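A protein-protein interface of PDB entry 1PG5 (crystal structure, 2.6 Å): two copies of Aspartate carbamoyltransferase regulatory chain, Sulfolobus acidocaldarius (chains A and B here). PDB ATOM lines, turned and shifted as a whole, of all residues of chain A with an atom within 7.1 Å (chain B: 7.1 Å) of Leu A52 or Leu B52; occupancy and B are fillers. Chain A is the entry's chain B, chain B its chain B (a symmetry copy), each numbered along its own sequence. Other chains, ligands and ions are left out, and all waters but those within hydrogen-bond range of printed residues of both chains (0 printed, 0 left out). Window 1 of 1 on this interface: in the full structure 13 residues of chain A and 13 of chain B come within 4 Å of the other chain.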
ATOM      1  N   MET A  15      15.893 -14.270   9.283  1.00  0.00           N
ATOM      2  CA  MET A  15      14.569 -14.845   9.698  1.00  0.00           C
ATOM      3  C   MET A  15      14.611 -15.417  11.169  1.00  0.00           C
ATOM      4  O   MET A  15      13.567 -15.748  11.720  1.00  0.00           O
ATOM      5  CB  MET A  15      14.124 -15.895   8.633  1.00  0.00           C
ATOM      6  CG  MET A  15      12.601 -16.120   8.486  1.00  0.00           C
ATOM      7  SD  MET A  15      12.131 -17.905   8.172  1.00  0.00           S
ATOM      8  CE  MET A  15      10.826 -18.378   9.507  1.00  0.00           C
ATOM      9  N   VAL A  16      15.812 -15.538  11.772  1.00  0.00           N
ATOM     10  CA  VAL A  16      16.033 -15.940  13.201  1.00  0.00           C
ATOM     11  C   VAL A  16      16.681 -14.849  14.147  1.00  0.00           C
ATOM     12  O   VAL A  16      17.475 -13.989  13.734  1.00  0.00           O
ATOM     13  CB  VAL A  16      16.910 -17.284  13.275  1.00  0.00           C
ATOM     14  CG1 VAL A  16      18.398 -17.027  12.999  1.00  0.00           C
ATOM     15  CG2 VAL A  16      16.716 -18.011  14.626  1.00  0.00           C
ATOM     16  N   ALA A  33      22.856 -26.848   5.303  1.00  0.00           N
ATOM     17  CA  ALA A  33      23.080 -26.617   6.703  1.00  0.00           C
ATOM     18  C   ALA A  33      23.222 -27.880   7.482  1.00  0.00           C
ATOM     19  O   ALA A  33      24.000 -27.873   8.463  1.00  0.00           O
ATOM     20  CB  ALA A  33      21.987 -25.827   7.309  1.00  0.00           C
ATOM     21  N   PHE A  34      22.501 -28.940   7.126  1.00  0.00           N
ATOM     22  CA  PHE A  34      22.574 -30.165   7.958  1.00  0.00           C
ATOM     23  C   PHE A  34      23.948 -30.754   7.821  1.00  0.00           C
ATOM     24  O   PHE A  34      24.494 -31.272   8.783  1.00  0.00           O
ATOM     25  CB  PHE A  34      21.491 -31.222   7.688  1.00  0.00           C
ATOM     26  CG  PHE A  34      20.124 -30.697   7.898  1.00  0.00           C
ATOM     27  CD1 PHE A  34      19.386 -30.241   6.805  1.00  0.00           C
ATOM     28  CD2 PHE A  34      19.612 -30.498   9.184  1.00  0.00           C
ATOM     29  CE1 PHE A  34      18.114 -29.660   7.012  1.00  0.00           C
ATOM     30  CE2 PHE A  34      18.334 -29.934   9.383  1.00  0.00           C
ATOM     31  CZ  PHE A  34      17.612 -29.513   8.327  1.00  0.00           C
ATOM     32  N   LEU A  37      26.628 -28.683  10.196  1.00  0.00           N
ATOM     33  CA  LEU A  37      26.579 -29.429  11.473  1.00  0.00           C
ATOM     34  C   LEU A  37      27.302 -30.803  11.536  1.00  0.00           C
ATOM     35  O   LEU A  37      28.056 -31.057  12.466  1.00  0.00           O
ATOM     36  CB  LEU A  37      25.115 -29.643  11.788  1.00  0.00           C
ATOM     37  CG  LEU A  37      24.255 -28.637  12.582  1.00  0.00           C
ATOM     38  CD1 LEU A  37      24.854 -27.249  12.649  1.00  0.00           C
ATOM     39  CD2 LEU A  37      22.838 -28.594  12.048  1.00  0.00           C
ATOM     40  N   ILE A  50      20.933 -24.168  19.203  1.00  0.00           N
ATOM     41  CA  ILE A  50      21.262 -24.006  17.806  1.00  0.00           C
ATOM     42  C   ILE A  50      20.015 -23.521  17.097  1.00  0.00           C
ATOM     43  O   ILE A  50      18.867 -23.907  17.406  1.00  0.00           O
ATOM     44  CB  ILE A  50      21.727 -25.377  17.183  1.00  0.00           C
ATOM     45  CG1 ILE A  50      23.000 -25.952  17.825  1.00  0.00           C
ATOM     46  CG2 ILE A  50      22.078 -25.292  15.709  1.00  0.00           C
ATOM     47  CD1 ILE A  50      22.959 -27.505  17.764  1.00  0.00           C
ATOM     48  N   ALA A  51      20.245 -22.674  16.115  1.00  0.00           N
ATOM     49  CA  ALA A  51      19.187 -22.352  15.203  1.00  0.00           C
ATOM     50  C   ALA A  51      19.651 -22.347  13.786  1.00  0.00           C
ATOM     51  O   ALA A  51      20.781 -21.989  13.480  1.00  0.00           O
ATOM     52  CB  ALA A  51      18.598 -21.053  15.518  1.00  0.00           C
ATOM     53  N   LEU A  52      18.734 -22.759  12.922  1.00  0.00           N
ATOM     54  CA  LEU A  52      18.935 -22.813  11.497  1.00  0.00           C
ATOM     55  C   LEU A  52      17.759 -22.154  10.769  1.00  0.00           C
ATOM     56  O   LEU A  52      16.613 -22.286  11.195  1.00  0.00           O
ATOM     57  CB  LEU A  52      18.831 -24.231  11.014  1.00  0.00           C
ATOM     58  CG  LEU A  52      19.301 -25.484  11.706  1.00  0.00           C
ATOM     59  CD1 LEU A  52      20.033 -26.266  10.670  1.00  0.00           C
ATOM     60  CD2 LEU A  52      20.236 -25.246  12.769  1.00  0.00           C
ATOM     61  N   VAL A  53      18.050 -21.545   9.630  1.00  0.00           N
ATOM     62  CA  VAL A  53      17.042 -21.359   8.629  1.00  0.00           C
ATOM     63  C   VAL A  53      17.599 -21.957   7.358  1.00  0.00           C
ATOM     64  O   VAL A  53      18.749 -21.775   7.046  1.00  0.00           O
ATOM     65  CB  VAL A  53      16.633 -19.853   8.522  1.00  0.00           C
ATOM     66  CG1 VAL A  53      16.326 -19.317   9.941  1.00  0.00           C
ATOM     67  CG2 VAL A  53      17.777 -19.034   7.980  1.00  0.00           C
ATOM     68  N   ILE A  54      16.733 -22.635   6.621  1.00  0.00           N
ATOM     69  CA  ILE A  54      17.076 -23.258   5.351  1.00  0.00           C
ATOM     70  C   ILE A  54      16.240 -22.690   4.208  1.00  0.00           C
ATOM     71  O   ILE A  54      15.045 -22.406   4.377  1.00  0.00           O
ATOM     72  CB  ILE A  54      16.814 -24.735   5.547  1.00  0.00           C
ATOM     73  CG1 ILE A  54      17.924 -25.290   6.398  1.00  0.00           C
ATOM     74  CG2 ILE A  54      16.690 -25.534   4.260  1.00  0.00           C
ATOM     75  CD1 ILE A  54      17.344 -26.237   7.440  1.00  0.00           C
ATOM     76  N   ASP A  65      21.301 -20.991   3.391  1.00  0.00           N
ATOM     77  CA  ASP A  65      21.067 -21.442   4.761  1.00  0.00           C
ATOM     78  C   ASP A  65      21.944 -20.614   5.768  1.00  0.00           C
ATOM     79  O   ASP A  65      22.984 -20.051   5.412  1.00  0.00           O
ATOM     80  CB  ASP A  65      21.379 -22.930   4.918  1.00  0.00           C
ATOM     81  CG  ASP A  65      20.519 -23.901   3.973  1.00  0.00           C
ATOM     82  OD1 ASP A  65      20.924 -25.126   3.850  1.00  0.00           O
ATOM     83  OD2 ASP A  65      19.426 -23.639   3.342  1.00  0.00           O
ATOM     84  N   ILE A  66      21.486 -20.561   7.016  1.00  0.00           N
ATOM     85  CA  ILE A  66      22.158 -19.903   8.111  1.00  0.00           C
ATOM     86  C   ILE A  66      22.085 -20.760   9.345  1.00  0.00           C
ATOM     87  O   ILE A  66      21.015 -21.192   9.716  1.00  0.00           O
ATOM     88  CB  ILE A  66      21.494 -18.551   8.462  1.00  0.00           C
ATOM     89  CG1 ILE A  66      21.458 -17.629   7.262  1.00  0.00           C
ATOM     90  CG2 ILE A  66      22.282 -17.833   9.531  1.00  0.00           C
ATOM     91  CD1 ILE A  66      20.610 -16.332   7.449  1.00  0.00           C
ATOM     92  N   VAL A  67      23.211 -20.933  10.020  1.00  0.00           N
ATOM     93  CA  VAL A  67      23.316 -21.691  11.256  1.00  0.00           C
ATOM     94  C   VAL A  67      23.857 -20.764  12.372  1.00  0.00           C
ATOM     95  O   VAL A  67      24.755 -19.975  12.160  1.00  0.00           O
ATOM     96  CB  VAL A  67      24.284 -22.846  11.037  1.00  0.00           C
ATOM     97  CG1 VAL A  67      24.591 -23.618  12.361  1.00  0.00           C
ATOM     98  CG2 VAL A  67      23.733 -23.783  10.017  1.00  0.00           C
ATOM     99  N   LYS A  68      23.310 -20.877  13.573  1.00  0.00           N
ATOM    100  CA  LYS A  68      23.727 -20.102  14.715  1.00  0.00           C
ATOM    101  C   LYS A  68      23.912 -21.092  15.852  1.00  0.00           C
ATOM    102  O   LYS A  68      23.029 -21.881  16.136  1.00  0.00           O
ATOM    103  CB  LYS A  68      22.620 -19.116  15.042  1.00  0.00           C
ATOM    104  CG  LYS A  68      22.578 -17.932  14.102  1.00  0.00           C
ATOM    105  CD  LYS A  68      21.445 -16.986  14.433  1.00  0.00           C
ATOM    106  CE  LYS A  68      21.488 -15.758  13.465  1.00  0.00           C
ATOM    107  NZ  LYS A  68      20.659 -14.535  13.855  1.00  0.00           N
ATOM    108  N   MET B  15      12.688 -17.974  19.874  1.00  0.00           N
ATOM    109  CA  MET B  15      14.040 -17.487  19.435  1.00  0.00           C
ATOM    110  C   MET B  15      14.114 -17.278  17.874  1.00  0.00           C
ATOM    111  O   MET B  15      15.082 -16.710  17.383  1.00  0.00           O
ATOM    112  CB  MET B  15      15.125 -18.465  19.986  1.00  0.00           C
ATOM    113  CG  MET B  15      16.530 -17.864  20.229  1.00  0.00           C
ATOM    114  SD  MET B  15      17.930 -19.027  19.793  1.00  0.00           S
ATOM    115  CE  MET B  15      19.085 -18.076  18.579  1.00  0.00           C
ATOM    116  N   VAL B  16      13.100 -17.754  17.118  1.00  0.00           N
ATOM    117  CA  VAL B  16      12.938 -17.538  15.642  1.00  0.00           C
ATOM    118  C   VAL B  16      11.679 -16.693  15.188  1.00  0.00           C
ATOM    119  O   VAL B  16      10.611 -16.688  15.822  1.00  0.00           O
ATOM    120  CB  VAL B  16      12.929 -18.946  14.868  1.00  0.00           C
ATOM    121  CG1 VAL B  16      11.597 -19.689  15.021  1.00  0.00           C
ATOM    122  CG2 VAL B  16      13.299 -18.772  13.376  1.00  0.00           C
ATOM    123  N   ALA B  33      14.290 -32.516  16.960  1.00  0.00           N
ATOM    124  CA  ALA B  33      13.786 -31.860  15.786  1.00  0.00           C
ATOM    125  C   ALA B  33      14.247 -32.505  14.522  1.00  0.00           C
ATOM    126  O   ALA B  33      13.463 -32.493  13.546  1.00  0.00           O
ATOM    127  CB  ALA B  33      14.180 -30.437  15.742  1.00  0.00           C
ATOM    128  N   PHE B  34      15.468 -33.030  14.475  1.00  0.00           N
ATOM    129  CA  PHE B  34      15.958 -33.585  13.191  1.00  0.00           C
ATOM    130  C   PHE B  34      15.158 -34.813  12.866  1.00  0.00           C
ATOM    131  O   PHE B  34      14.854 -35.061  11.708  1.00  0.00           O
ATOM    132  CB  PHE B  34      17.465 -33.874  13.118  1.00  0.00           C
ATOM    133  CG  PHE B  34      18.284 -32.664  13.349  1.00  0.00           C
ATOM    134  CD1 PHE B  34      18.801 -32.413  14.622  1.00  0.00           C
ATOM    135  CD2 PHE B  34      18.423 -31.681  12.363  1.00  0.00           C
ATOM    136  CE1 PHE B  34      19.510 -31.216  14.867  1.00  0.00           C
ATOM    137  CE2 PHE B  34      19.149 -30.497  12.609  1.00  0.00           C
ATOM    138  CZ  PHE B  34      19.665 -30.263  13.831  1.00  0.00           C
ATOM    139  N   LEU B  37      11.486 -33.743  11.289  1.00  0.00           N
ATOM    140  CA  LEU B  37      11.755 -33.695   9.835  1.00  0.00           C
ATOM    141  C   LEU B  37      11.892 -35.045   9.079  1.00  0.00           C
ATOM    142  O   LEU B  37      11.276 -35.231   8.038  1.00  0.00           O
ATOM    143  CB  LEU B  37      13.040 -32.916   9.663  1.00  0.00           C
ATOM    144  CG  LEU B  37      13.098 -31.381   9.514  1.00  0.00           C
ATOM    145  CD1 LEU B  37      11.840 -30.680   9.979  1.00  0.00           C
ATOM    146  CD2 LEU B  37      14.322 -30.815  10.204  1.00  0.00           C
ATOM    147  N   ILE B  50      12.514 -23.481   6.038  1.00  0.00           N
ATOM    148  CA  ILE B  50      12.346 -24.153   7.305  1.00  0.00           C
ATOM    149  C   ILE B  50      13.213 -23.438   8.319  1.00  0.00           C
ATOM    150  O   ILE B  50      14.331 -22.958   8.035  1.00  0.00           O
ATOM    151  CB  ILE B  50      12.789 -25.662   7.196  1.00  0.00           C
ATOM    152  CG1 ILE B  50      11.960 -26.484   6.199  1.00  0.00           C
ATOM    153  CG2 ILE B  50      12.657 -26.434   8.496  1.00  0.00           C
ATOM    154  CD1 ILE B  50      12.844 -27.603   5.582  1.00  0.00           C
ATOM    155  N   ALA B  51      12.698 -23.383   9.530  1.00  0.00           N
ATOM    156  CA  ALA B  51      13.527 -22.976  10.628  1.00  0.00           C
ATOM    157  C   ALA B  51      13.335 -23.843  11.825  1.00  0.00           C
ATOM    158  O   ALA B  51      12.247 -24.334  12.099  1.00  0.00           O
ATOM    159  CB  ALA B  51      13.267 -21.587  10.996  1.00  0.00           C
ATOM    160  N   LEU B  52      14.438 -24.019  12.541  1.00  0.00           N
ATOM    161  CA  LEU B  52      14.497 -24.789  13.757  1.00  0.00           C
ATOM    162  C   LEU B  52      15.214 -23.996  14.854  1.00  0.00           C
ATOM    163  O   LEU B  52      16.177 -23.283  14.575  1.00  0.00           O
ATOM    164  CB  LEU B  52      15.419 -25.961  13.581  1.00  0.00           C
ATOM    165  CG  LEU B  52      15.613 -26.814  12.353  1.00  0.00           C
ATOM    166  CD1 LEU B  52      15.574 -28.224  12.832  1.00  0.00           C
ATOM    167  CD2 LEU B  52      14.562 -26.686  11.384  1.00  0.00           C
ATOM    168  N   VAL B  53      14.800 -24.214  16.091  1.00  0.00           N
ATOM    169  CA  VAL B  53      15.672 -23.971  17.201  1.00  0.00           C
ATOM    170  C   VAL B  53      15.710 -25.257  17.994  1.00  0.00           C
ATOM    171  O   VAL B  53      14.701 -25.886  18.192  1.00  0.00           O
ATOM    172  CB  VAL B  53      15.209 -22.714  18.010  1.00  0.00           C
ATOM    173  CG1 VAL B  53      14.976 -21.543  17.025  1.00  0.00           C
ATOM    174  CG2 VAL B  53      13.891 -22.984  18.692  1.00  0.00           C
ATOM    175  N   ILE B  54      16.897 -25.595  18.471  1.00  0.00           N
ATOM    176  CA  ILE B  54      17.126 -26.783  19.282  1.00  0.00           C
ATOM    177  C   ILE B  54      17.668 -26.421  20.661  1.00  0.00           C
ATOM    178  O   ILE B  54      18.481 -25.495  20.799  1.00  0.00           O
ATOM    179  CB  ILE B  54      18.118 -27.616  18.499  1.00  0.00           C
ATOM    180  CG1 ILE B  54      17.382 -28.245  17.347  1.00  0.00           C
ATOM    181  CG2 ILE B  54      18.831 -28.684  19.311  1.00  0.00           C
ATOM    182  CD1 ILE B  54      18.232 -28.155  16.088  1.00  0.00           C
ATOM    183  N   ASP B  65      12.666 -28.304  21.432  1.00  0.00           N
ATOM    184  CA  ASP B  65      12.914 -27.903  20.049  1.00  0.00           C
ATOM    185  C   ASP B  65      11.600 -27.344  19.394  1.00  0.00           C
ATOM    186  O   ASP B  65      10.483 -27.660  19.814  1.00  0.00           O
ATOM    187  CB  ASP B  65      13.442 -29.071  19.216  1.00  0.00           C
ATOM    188  CG  ASP B  65      14.812 -29.714  19.751  1.00  0.00           C
ATOM    189  OD1 ASP B  65      15.159 -30.866  19.270  1.00  0.00           O
ATOM    190  OD2 ASP B  65      15.662 -29.208  20.578  1.00  0.00           O
ATOM    191  N   ILE B  66      11.779 -26.513  18.370  1.00  0.00           N
ATOM    192  CA  ILE B  66      10.714 -25.927  17.591  1.00  0.00           C
ATOM    193  C   ILE B  66      11.069 -25.964  16.131  1.00  0.00           C
ATOM    194  O   ILE B  66      12.139 -25.531  15.759  1.00  0.00           O
ATOM    195  CB  ILE B  66      10.482 -24.444  17.962  1.00  0.00           C
ATOM    196  CG1 ILE B  66      10.178 -24.287  19.437  1.00  0.00           C
ATOM    197  CG2 ILE B  66       9.294 -23.889  17.216  1.00  0.00           C
ATOM    198  CD1 ILE B  66      10.151 -22.813  19.953  1.00  0.00           C
ATOM    199  N   VAL B  67      10.138 -26.404  15.300  1.00  0.00           N
ATOM    200  CA  VAL B  67      10.291 -26.466  13.857  1.00  0.00           C
ATOM    201  C   VAL B  67       9.186 -25.607  13.194  1.00  0.00           C
ATOM    202  O   VAL B  67       8.043 -25.620  13.603  1.00  0.00           O
ATOM    203  CB  VAL B  67      10.145 -27.915  13.412  1.00  0.00           C
ATOM    204  CG1 VAL B  67      10.127 -28.058  11.857  1.00  0.00           C
ATOM    205  CG2 VAL B  67      11.251 -28.734  13.987  1.00  0.00           C
ATOM    206  N   LYS B  68       9.534 -24.867  12.152  1.00  0.00           N
ATOM    207  CA  LYS B  68       8.611 -24.038  11.417  1.00  0.00           C
ATOM    208  C   LYS B  68       8.839 -24.352   9.950  1.00  0.00           C
ATOM    209  O   LYS B  68       9.959 -24.316   9.475  1.00  0.00           O
ATOM    210  CB  LYS B  68       8.948 -22.587  11.710  1.00  0.00           C
ATOM    211  CG  LYS B  68       8.471 -22.125  13.069  1.00  0.00           C
ATOM    212  CD  LYS B  68       8.851 -20.687  13.343  1.00  0.00           C
ATOM    213  CE  LYS B  68       8.282 -20.251  14.734  1.00  0.00           C
ATOM    214  NZ  LYS B  68       8.253 -18.754  15.037  1.00  0.00           N
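Of the 14 printed residues of chain B, 8 touch a printed residue of chain A. Hydrophobic or aromatic side chains of chain B within 4 Å of the printed part of chain A: Val B16, Phe B34, Ala B51, Leu B52, Val B53 and Ile B54. Hydrophobic or aromatic side chains of chain A within 4 Å of the printed part of chain B: Val A16, Phe A34, Ala A51, Leu A52, Val A53 and Ile A54. Among the printed residues, 15 pairs touch across the chains.
Met A15 touches Val B16, and with the chains exchanged Val A16 touches Met B15. Ile A50 touches Val B53, and with the chains exchanged Val A53 touches Ile B50. Ala A51 touches Leu B52, and with the chains exchanged Leu A52 touches Ala B51. Leu B52 touches its own counterpart, Leu A52. Positions printed for both chains: 15, 16, 33, 34, 37, 50, 51, 52, 53, 54, 65, 66, 67 and 68. Of the 15 pairs that touch across the chains among the printed residues, 15 have their exchanged pair printed and touching as well.
Leu A52 touches three residues of chain B. Of the printed residues of chain A, Leu B52 touches Ile A50 (3.95 Å), Ala A51 (3.2 Å) and Leu A52 (3.1 Å). Of the printed residues of chain A, Ile B50 touches Leu A52, Val A53 and Ile A54. Of the printed residues of chain A, Phe B34 touches Phe A34. Of the printed residues of chain A, Ile B54 touches Ile A50. Of the printed residues of chain B, Val A53 touches Ile B50 and Ala B51. The nearest residue of chain B that does not touch Leu A52 is Phe B34 (4.7 Å). The nearest residue of chain A that does not touch Leu B52 is Phe A34 (4.7 Å).
O of Ala A51 lies within hydrogen-bond range of N of Lys A68 (2.8 Å). The backbone carbonyl oxygen of Ile B66 sits at hydrogen-bond distance from the backbone NH of Val B53, at 3.0 Å. The side-chain amino group (NZ) of Lys A68 sits at hydrogen-bond distance from the backbone carbonyl oxygen (O) of Val A16 (3.2 Å). The backbone carbonyl oxygen (O) of Val B16 sits at hydrogen-bond distance from the side-chain amino group (NZ) of Lys B68 (3.2 Å). N of Lys B68 lies within hydrogen-bond range of O of Ala B51 (2.8 Å). The backbone carbonyl oxygen (O) of Ile A66 sits at hydrogen-bond distance from the backbone NH (N) of Val A53.
Among the printed residues, merely in contact across the chains: Ile A50 with Val B53 (3.2 Å), Val A53 with Ile B50 (3.2 Å), Leu A52 with Ala B51 (3.2 Å), Ala A51 with Leu B52 (3.2 Å), Phe A34 with Phe B34 (3.4 Å), Met A15 with Val B16 (3.5 Å), Val A16 with Met B15 (3.5 Å), Val A16 with Val B16 (3.7 Å), Val A53 with Ala B51 (3.95 Å), Ala A51 with Val B53 (3.95 Å), Ile A50 with Leu B52 (3.95 Å) and Leu A52 with Ile B50 (3.96 Å).
N of Ile A54 lies within hydrogen-bond range of O of Ile B50, 2.8 Å away. The backbone NH (N) of Leu A52 is in hydrogen-bond range of the backbone carbonyl oxygen (O) of Leu B52 (3.1 Å). N of Ile B54 lies within hydrogen-bond range of O of Ile A50 (2.8 Å).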
